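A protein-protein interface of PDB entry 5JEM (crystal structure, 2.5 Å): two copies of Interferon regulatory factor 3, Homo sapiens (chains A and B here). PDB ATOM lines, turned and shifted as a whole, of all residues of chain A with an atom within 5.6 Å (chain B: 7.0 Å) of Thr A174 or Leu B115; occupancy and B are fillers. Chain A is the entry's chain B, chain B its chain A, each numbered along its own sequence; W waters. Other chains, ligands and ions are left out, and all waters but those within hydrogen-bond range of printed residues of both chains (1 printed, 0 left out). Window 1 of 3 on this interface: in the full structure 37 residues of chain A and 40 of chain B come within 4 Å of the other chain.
OE2 of Glu B203 lies within salt-bridge range of NH2 of Arg A26, at 2.5 Å. OG1 of Thr A174 sits at hydrogen-bond distance from OE1 of Glu B112 (3.3 Å). OE2 of Glu B112 is in salt-bridge range of NZ of Lys A175, at 2.6 Å.
The guanidinium group (NH1) of Arg A26 lies within hydrogen-bond range of the backbone carbonyl oxygen (O) of Lys A175, at 2.6 Å. The backbone NH (N) of Arg A26 is in hydrogen-bond range of the backbone carbonyl oxygen (O) of Arg A176 (3.1 Å). O of Leu B115 lies within hydrogen-bond range of OG of Ser B111. The backbone carbonyl oxygen (O) of Glu B112 lies within hydrogen-bond range of the indole nitrogen (NE1) of Trp B160 (2.9 Å).
Arg A26 touches Leu B114. Leu B114 touches Gly A27 (CD1 to C, 3.4 Å). Leu B115 touches Pro A172 (CD2 to CB, 3.7 Å). Thr A174 touches Leu B115 (CG2 to CD2, 3.97 Å). OE2 of Glu B203 touches CD of Lys A175, at 3.4 Å.
Thr A174 touches just these residues of chain B: Glu B112 and Leu B115. Of the printed residues of chain A, Leu B115 touches Pro A172 and Thr A174. Printed residues of chain B within 4 Å of Lys A175: Glu B112 and Glu B203. Of the printed residues of chain B, Arg A26 touches Leu B114 (3.8 Å) and Glu B203 (2.5 Å). Printed residues of chain B within 4 Å of Pro A172: Leu B115. Printed residues of chain B within 4 Å of Gly A27: Leu B114 (3.4 Å). Trp A173 touches none of the printed residues of chain B. Pro B116 touches none of the printed residues of chain A. The nearest residue of chain B that does not touch Thr A174 is Leu B114 (4.4 Å).
Of the 14 printed residues of chain B, 4 touch a printed residue of chain A. Hydrophobic or aromatic side chains of chain B that line the printed part of chain A: Leu B114 and Leu B115. Among the printed residues, 8 pairs touch across the chains. Among the printed residues, Asp or Glu carboxylates within 4 Å of a Lys or Arg side-chain nitrogen of the other chain: Arg A26 with Glu B203 (2.5 Å) and Lys A175 with Glu B112 (2.6 Å).
Thr A174 touches Leu B115, but with the chains exchanged Leu A115 does not touch Thr B174 (4.1 Å). Of the 8 pairs that touch across the chains among the printed residues, none has its exchanged pair printed and touching as well.
Water W1 bridges NZ of Lys A175 (2.4 Å) and OE2 of Glu B112 (2.7 Å).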
ATOM      1  N   ARG A  26     -34.462  -6.341  15.654  1.00  0.00           N
ATOM      2  CA  ARG A  26     -33.096  -5.831  15.688  1.00  0.00           C
ATOM      3  C   ARG A  26     -33.058  -4.473  16.395  1.00  0.00           C
ATOM      4  O   ARG A  26     -32.408  -3.531  15.942  1.00  0.00           O
ATOM      5  CB  ARG A  26     -32.536  -5.741  14.262  1.00  0.00           C
ATOM      6  CG  ARG A  26     -31.032  -5.543  14.151  1.00  0.00           C
ATOM      7  CD  ARG A  26     -30.242  -6.793  14.490  1.00  0.00           C
ATOM      8  NE  ARG A  26     -28.824  -6.591  14.207  1.00  0.00           N
ATOM      9  CZ  ARG A  26     -27.882  -7.506  14.403  1.00  0.00           C
ATOM     10  NH1 ARG A  26     -28.205  -8.696  14.889  1.00  0.00           N
ATOM     11  NH2 ARG A  26     -26.617  -7.229  14.114  1.00  0.00           N
ATOM     12  N   GLY A  27     -33.791  -4.380  17.503  1.00  0.00           N
ATOM     13  CA  GLY A  27     -33.815  -3.176  18.313  1.00  0.00           C
ATOM     14  C   GLY A  27     -34.893  -2.176  17.936  1.00  0.00           C
ATOM     15  O   GLY A  27     -35.386  -1.437  18.786  1.00  0.00           O
ATOM     16  N   LEU A 115     -36.273  -1.449  29.048  1.00  0.00           N
ATOM     17  CA  LEU A 115     -35.063  -2.226  28.803  1.00  0.00           C
ATOM     18  C   LEU A 115     -35.180  -3.625  29.397  1.00  0.00           C
ATOM     19  O   LEU A 115     -35.438  -3.772  30.591  1.00  0.00           O
ATOM     20  CB  LEU A 115     -33.846  -1.503  29.389  1.00  0.00           C
ATOM     21  CG  LEU A 115     -32.525  -1.528  28.618  1.00  0.00           C
ATOM     22  CD1 LEU A 115     -32.690  -0.895  27.246  1.00  0.00           C
ATOM     23  CD2 LEU A 115     -31.436  -0.811  29.403  1.00  0.00           C
ATOM     24  N   PRO A 172     -25.912  -6.746  23.706  1.00  0.00           N
ATOM     25  CA  PRO A 172     -27.039  -5.806  23.729  1.00  0.00           C
ATOM     26  C   PRO A 172     -28.283  -6.417  23.094  1.00  0.00           C
ATOM     27  O   PRO A 172     -28.172  -7.112  22.084  1.00  0.00           O
ATOM     28  CB  PRO A 172     -26.525  -4.618  22.913  1.00  0.00           C
ATOM     29  CG  PRO A 172     -25.478  -5.193  22.029  1.00  0.00           C
ATOM     30  CD  PRO A 172     -24.827  -6.285  22.825  1.00  0.00           C
ATOM     31  N   TRP A 173     -29.451  -6.157  23.674  1.00  0.00           N
ATOM     32  CA  TRP A 173     -30.687  -6.793  23.220  1.00  0.00           C
ATOM     33  C   TRP A 173     -31.073  -6.367  21.808  1.00  0.00           C
ATOM     34  O   TRP A 173     -31.890  -7.016  21.158  1.00  0.00           O
ATOM     35  CB  TRP A 173     -31.834  -6.485  24.185  1.00  0.00           C
ATOM     36  CG  TRP A 173     -32.292  -5.059  24.159  1.00  0.00           C
ATOM     37  CD1 TRP A 173     -31.746  -4.009  24.839  1.00  0.00           C
ATOM     38  CD2 TRP A 173     -33.403  -4.526  23.425  1.00  0.00           C
ATOM     39  NE1 TRP A 173     -32.443  -2.855  24.569  1.00  0.00           N
ATOM     40  CE2 TRP A 173     -33.465  -3.145  23.704  1.00  0.00           C
ATOM     41  CE3 TRP A 173     -34.347  -5.080  22.555  1.00  0.00           C
ATOM     42  CZ2 TRP A 173     -34.433  -2.312  23.146  1.00  0.00           C
ATOM     43  CZ3 TRP A 173     -35.309  -4.251  22.002  1.00  0.00           C
ATOM     44  CH2 TRP A 173     -35.345  -2.883  22.299  1.00  0.00           C
ATOM     45  N   THR A 174     -30.476  -5.279  21.336  1.00  0.00           N
ATOM     46  CA  THR A 174     -30.746  -4.790  19.991  1.00  0.00           C
ATOM     47  C   THR A 174     -30.125  -5.703  18.931  1.00  0.00           C
ATOM     48  O   THR A 174     -30.447  -5.590  17.749  1.00  0.00           O
ATOM     49  CB  THR A 174     -30.227  -3.351  19.801  1.00  0.00           C
ATOM     50  OG1 THR A 174     -28.795  -3.354  19.724  1.00  0.00           O
ATOM     51  CG2 THR A 174     -30.674  -2.471  20.963  1.00  0.00           C
ATOM     52  N   LYS A 175     -29.239  -6.603  19.358  1.00  0.00           N
ATOM     53  CA  LYS A 175     -28.642  -7.583  18.449  1.00  0.00           C
ATOM     54  C   LYS A 175     -29.623  -8.689  18.099  1.00  0.00           C
ATOM     55  O   LYS A 175     -29.445  -9.388  17.107  1.00  0.00           O
ATOM     56  CB  LYS A 175     -27.380  -8.210  19.050  1.00  0.00           C
ATOM     57  CG  LYS A 175     -26.189  -7.273  19.148  1.00  0.00           C
ATOM     58  CD  LYS A 175     -25.950  -6.526  17.845  1.00  0.00           C
ATOM     59  CE  LYS A 175     -25.072  -5.303  18.078  1.00  0.00           C
ATOM     60  NZ  LYS A 175     -24.981  -4.421  16.881  1.00  0.00           N
ATOM     61  N   ARG A 176     -30.651  -8.855  18.923  1.00  0.00           N
ATOM     62  CA  ARG A 176     -31.615  -9.926  18.717  1.00  0.00           C
ATOM     63  C   ARG A 176     -32.556  -9.609  17.566  1.00  0.00           C
ATOM     64  O   ARG A 176     -32.951  -8.464  17.368  1.00  0.00           O
ATOM     65  CB  ARG A 176     -32.403 -10.191  20.001  1.00  0.00           C
ATOM     66  CG  ARG A 176     -31.594 -10.926  21.058  1.00  0.00           C
ATOM     67  CD  ARG A 176     -30.948 -12.171  20.464  1.00  0.00           C
ATOM     68  NE  ARG A 176     -30.150 -12.910  21.436  1.00  0.00           N
ATOM     69  CZ  ARG A 176     -28.823 -12.863  21.507  1.00  0.00           C
ATOM     70  NH1 ARG A 176     -28.137 -12.110  20.657  1.00  0.00           N
ATOM     71  NH2 ARG A 176     -28.182 -13.572  22.425  1.00  0.00           N
ATOM     72  N   SER B 111     -22.126   6.357  18.876  1.00  0.00           N
ATOM     73  CA  SER B 111     -22.613   5.011  19.143  1.00  0.00           C
ATOM     74  C   SER B 111     -23.679   4.554  18.153  1.00  0.00           C
ATOM     75  O   SER B 111     -23.874   5.167  17.102  1.00  0.00           O
ATOM     76  CB  SER B 111     -23.164   4.934  20.569  1.00  0.00           C
ATOM     77  OG  SER B 111     -23.425   3.594  20.942  1.00  0.00           O
ATOM     78  N   GLU B 112     -24.355   3.462  18.496  1.00  0.00           N
ATOM     79  CA  GLU B 112     -25.481   2.972  17.710  1.00  0.00           C
ATOM     80  C   GLU B 112     -26.645   3.948  17.787  1.00  0.00           C
ATOM     81  O   GLU B 112     -26.666   4.852  18.625  1.00  0.00           O
ATOM     82  CB  GLU B 112     -25.933   1.591  18.192  1.00  0.00           C
ATOM     83  CG  GLU B 112     -25.070   0.429  17.730  1.00  0.00           C
ATOM     84  CD  GLU B 112     -25.669  -0.912  18.112  1.00  0.00           C
ATOM     85  OE1 GLU B 112     -26.680  -0.925  18.850  1.00  0.00           O
ATOM     86  OE2 GLU B 112     -25.134  -1.953  17.674  1.00  0.00           O
ATOM     87  N   GLU B 113     -27.625   3.751  16.916  1.00  0.00           N
ATOM     88  CA  GLU B 113     -28.757   4.658  16.851  1.00  0.00           C
ATOM     89  C   GLU B 113     -29.768   4.378  17.963  1.00  0.00           C
ATOM     90  O   GLU B 113     -30.567   5.244  18.318  1.00  0.00           O
ATOM     91  CB  GLU B 113     -29.428   4.561  15.481  1.00  0.00           C
ATOM     92  CG  GLU B 113     -30.311   5.745  15.155  1.00  0.00           C
ATOM     93  CD  GLU B 113     -30.398   6.010  13.672  1.00  0.00           C
ATOM     94  OE1 GLU B 113     -31.210   6.867  13.270  1.00  0.00           O
ATOM     95  OE2 GLU B 113     -29.651   5.366  12.910  1.00  0.00           O
ATOM     96  N   LEU B 114     -29.714   3.175  18.524  1.00  0.00           N
ATOM     97  CA  LEU B 114     -30.735   2.733  19.467  1.00  0.00           C
ATOM     98  C   LEU B 114     -30.218   2.574  20.893  1.00  0.00           C
ATOM     99  O   LEU B 114     -30.998   2.559  21.847  1.00  0.00           O
ATOM    100  CB  LEU B 114     -31.340   1.412  18.993  1.00  0.00           C
ATOM    101  CG  LEU B 114     -31.954   1.476  17.595  1.00  0.00           C
ATOM    102  CD1 LEU B 114     -32.460   0.113  17.151  1.00  0.00           C
ATOM    103  CD2 LEU B 114     -33.074   2.503  17.563  1.00  0.00           C
ATOM    104  N   LEU B 115     -28.903   2.461  21.042  1.00  0.00           N
ATOM    105  CA  LEU B 115     -28.317   2.189  22.346  1.00  0.00           C
ATOM    106  C   LEU B 115     -26.980   2.898  22.490  1.00  0.00           C
ATOM    107  O   LEU B 115     -26.033   2.576  21.776  1.00  0.00           O
ATOM    108  CB  LEU B 115     -28.144   0.679  22.536  1.00  0.00           C
ATOM    109  CG  LEU B 115     -28.425   0.072  23.911  1.00  0.00           C
ATOM    110  CD1 LEU B 115     -29.845   0.386  24.365  1.00  0.00           C
ATOM    111  CD2 LEU B 115     -28.190  -1.432  23.874  1.00  0.00           C
ATOM    112  N   PRO B 116     -26.896   3.868  23.417  1.00  0.00           N
ATOM    113  CA  PRO B 116     -25.647   4.597  23.676  1.00  0.00           C
ATOM    114  C   PRO B 116     -24.546   3.674  24.199  1.00  0.00           C
ATOM    115  O   PRO B 116     -23.365   4.009  24.098  1.00  0.00           O
ATOM    116  CB  PRO B 116     -26.053   5.631  24.730  1.00  0.00           C
ATOM    117  CG  PRO B 116     -27.272   5.073  25.362  1.00  0.00           C
ATOM    118  CD  PRO B 116     -27.991   4.323  24.289  1.00  0.00           C
ATOM    119  N   ASN B 117     -24.955   2.536  24.759  1.00  0.00           N
ATOM    120  CA  ASN B 117     -24.066   1.422  25.108  1.00  0.00           C
ATOM    121  C   ASN B 117     -23.044   1.693  26.212  1.00  0.00           C
ATOM    122  O   ASN B 117     -22.663   2.835  26.472  1.00  0.00           O
ATOM    123  CB  ASN B 117     -23.329   0.932  23.857  1.00  0.00           C
ATOM    124  CG  ASN B 117     -24.218   0.119  22.936  1.00  0.00           C
ATOM    125  OD1 ASN B 117     -24.485  -1.056  23.192  1.00  0.00           O
ATOM    126  ND2 ASN B 117     -24.675   0.737  21.853  1.00  0.00           N
ATOM    127  N   SER B 118     -22.606   0.608  26.846  1.00  0.00           N
ATOM    128  CA  SER B 118     -21.683   0.647  27.977  1.00  0.00           C
ATOM    129  C   SER B 118     -21.177  -0.767  28.271  1.00  0.00           C
ATOM    130  O   SER B 118     -21.885  -1.740  28.015  1.00  0.00           O
ATOM    131  CB  SER B 118     -22.371   1.246  29.210  1.00  0.00           C
ATOM    132  OG  SER B 118     -22.573   2.640  29.052  1.00  0.00           O
ATOM    133  N   HIS B 120     -17.842   0.847  27.218  1.00  0.00           N
ATOM    134  CA  HIS B 120     -16.613   1.183  26.516  1.00  0.00           C
ATOM    135  C   HIS B 120     -16.238   2.618  26.866  1.00  0.00           C
ATOM    136  O   HIS B 120     -15.282   3.177  26.327  1.00  0.00           O
ATOM    137  CB  HIS B 120     -16.770   1.005  25.004  1.00  0.00           C
ATOM    138  CG  HIS B 120     -18.034   1.585  24.452  1.00  0.00           C
ATOM    139  ND1 HIS B 120     -19.073   0.803  23.995  1.00  0.00           N
ATOM    140  CD2 HIS B 120     -18.429   2.870  24.283  1.00  0.00           C
ATOM    141  CE1 HIS B 120     -20.052   1.581  23.567  1.00  0.00           C
ATOM    142  NE2 HIS B 120     -19.687   2.839  23.733  1.00  0.00           N
ATOM    143  N   TRP B 160     -24.515  10.666  21.117  1.00  0.00           N
ATOM    144  CA  TRP B 160     -25.299  10.657  22.342  1.00  0.00           C
ATOM    145  C   TRP B 160     -24.693  11.601  23.371  1.00  0.00           C
ATOM    146  O   TRP B 160     -23.475  11.665  23.525  1.00  0.00           O
ATOM    147  CB  TRP B 160     -25.391   9.243  22.911  1.00  0.00           C
ATOM    148  CG  TRP B 160     -26.316   8.350  22.149  1.00  0.00           C
ATOM    149  CD1 TRP B 160     -26.039   7.670  20.999  1.00  0.00           C
ATOM    150  CD2 TRP B 160     -27.669   8.030  22.489  1.00  0.00           C
ATOM    151  NE1 TRP B 160     -27.138   6.949  20.600  1.00  0.00           N
ATOM    152  CE2 TRP B 160     -28.151   7.152  21.499  1.00  0.00           C
ATOM    153  CE3 TRP B 160     -28.521   8.401  23.533  1.00  0.00           C
ATOM    154  CZ2 TRP B 160     -29.446   6.638  21.524  1.00  0.00           C
ATOM    155  CZ3 TRP B 160     -29.807   7.891  23.555  1.00  0.00           C
ATOM    156  CH2 TRP B 160     -30.256   7.020  22.557  1.00  0.00           C
ATOM    157  N   TRP B 173     -28.450   3.205  30.677  1.00  0.00           N
ATOM    158  CA  TRP B 173     -28.544   4.614  30.311  1.00  0.00           C
ATOM    159  C   TRP B 173     -29.917   5.191  30.642  1.00  0.00           C
ATOM    160  O   TRP B 173     -30.088   6.409  30.724  1.00  0.00           O
ATOM    161  CB  TRP B 173     -28.247   4.787  28.822  1.00  0.00           C
ATOM    162  CG  TRP B 173     -29.286   4.158  27.949  1.00  0.00           C
ATOM    163  CD1 TRP B 173     -29.368   2.844  27.583  1.00  0.00           C
ATOM    164  CD2 TRP B 173     -30.400   4.815  27.339  1.00  0.00           C
ATOM    165  NE1 TRP B 173     -30.466   2.645  26.780  1.00  0.00           N
ATOM    166  CE2 TRP B 173     -31.116   3.840  26.615  1.00  0.00           C
ATOM    167  CE3 TRP B 173     -30.865   6.135  27.336  1.00  0.00           C
ATOM    168  CZ2 TRP B 173     -32.269   4.143  25.893  1.00  0.00           C
ATOM    169  CZ3 TRP B 173     -32.008   6.434  26.619  1.00  0.00           C
ATOM    170  CH2 TRP B 173     -32.698   5.443  25.907  1.00  0.00           C
ATOM    171  N   THR B 174     -30.889   4.303  30.834  1.00  0.00           N
ATOM    172  CA  THR B 174     -32.252   4.700  31.161  1.00  0.00           C
ATOM    173  C   THR B 174     -32.358   5.261  32.577  1.00  0.00           C
ATOM    174  O   THR B 174     -33.392   5.803  32.958  1.00  0.00           O
ATOM    175  CB  THR B 174     -33.226   3.519  31.017  1.00  0.00           C
ATOM    176  OG1 THR B 174     -32.927   2.523  32.002  1.00  0.00           O
ATOM    177  CG2 THR B 174     -33.112   2.908  29.627  1.00  0.00           C
ATOM    178  N   LYS B 181     -29.923  12.159  21.916  1.00  0.00           N
ATOM    179  CA  LYS B 181     -29.322  11.599  20.712  1.00  0.00           C
ATOM    180  C   LYS B 181     -29.463  12.563  19.545  1.00  0.00           C
ATOM    181  O   LYS B 181     -30.547  13.086  19.286  1.00  0.00           O
ATOM    182  CB  LYS B 181     -29.951  10.256  20.339  1.00  0.00           C
ATOM    183  CG  LYS B 181     -29.451   9.727  18.995  1.00  0.00           C
ATOM    184  CD  LYS B 181     -30.100   8.414  18.591  1.00  0.00           C
ATOM    185  CE  LYS B 181     -31.517   8.616  18.089  1.00  0.00           C
ATOM    186  NZ  LYS B 181     -32.060   7.396  17.423  1.00  0.00           N
ATOM    187  N   GLU B 203     -24.386 -10.501  12.049  1.00  0.00           N
ATOM    188  CA  GLU B 203     -23.159 -11.199  12.407  1.00  0.00           C
ATOM    189  C   GLU B 203     -23.225 -12.643  11.937  1.00  0.00           C
ATOM    190  O   GLU B 203     -24.307 -13.207  11.807  1.00  0.00           O
ATOM    191  CB  GLU B 203     -22.924 -11.151  13.919  1.00  0.00           C
ATOM    192  CG  GLU B 203     -22.993  -9.757  14.528  1.00  0.00           C
ATOM    193  CD  GLU B 203     -24.415  -9.305  14.811  1.00  0.00           C
ATOM    194  OE1 GLU B 203     -25.349 -10.112  14.611  1.00  0.00           O
ATOM    195  OE2 GLU B 203     -24.598  -8.142  15.232  1.00  0.00           O
HETATM  196  O   HOH W   1     -26.721  -3.089  15.858  1.00  0.00           O
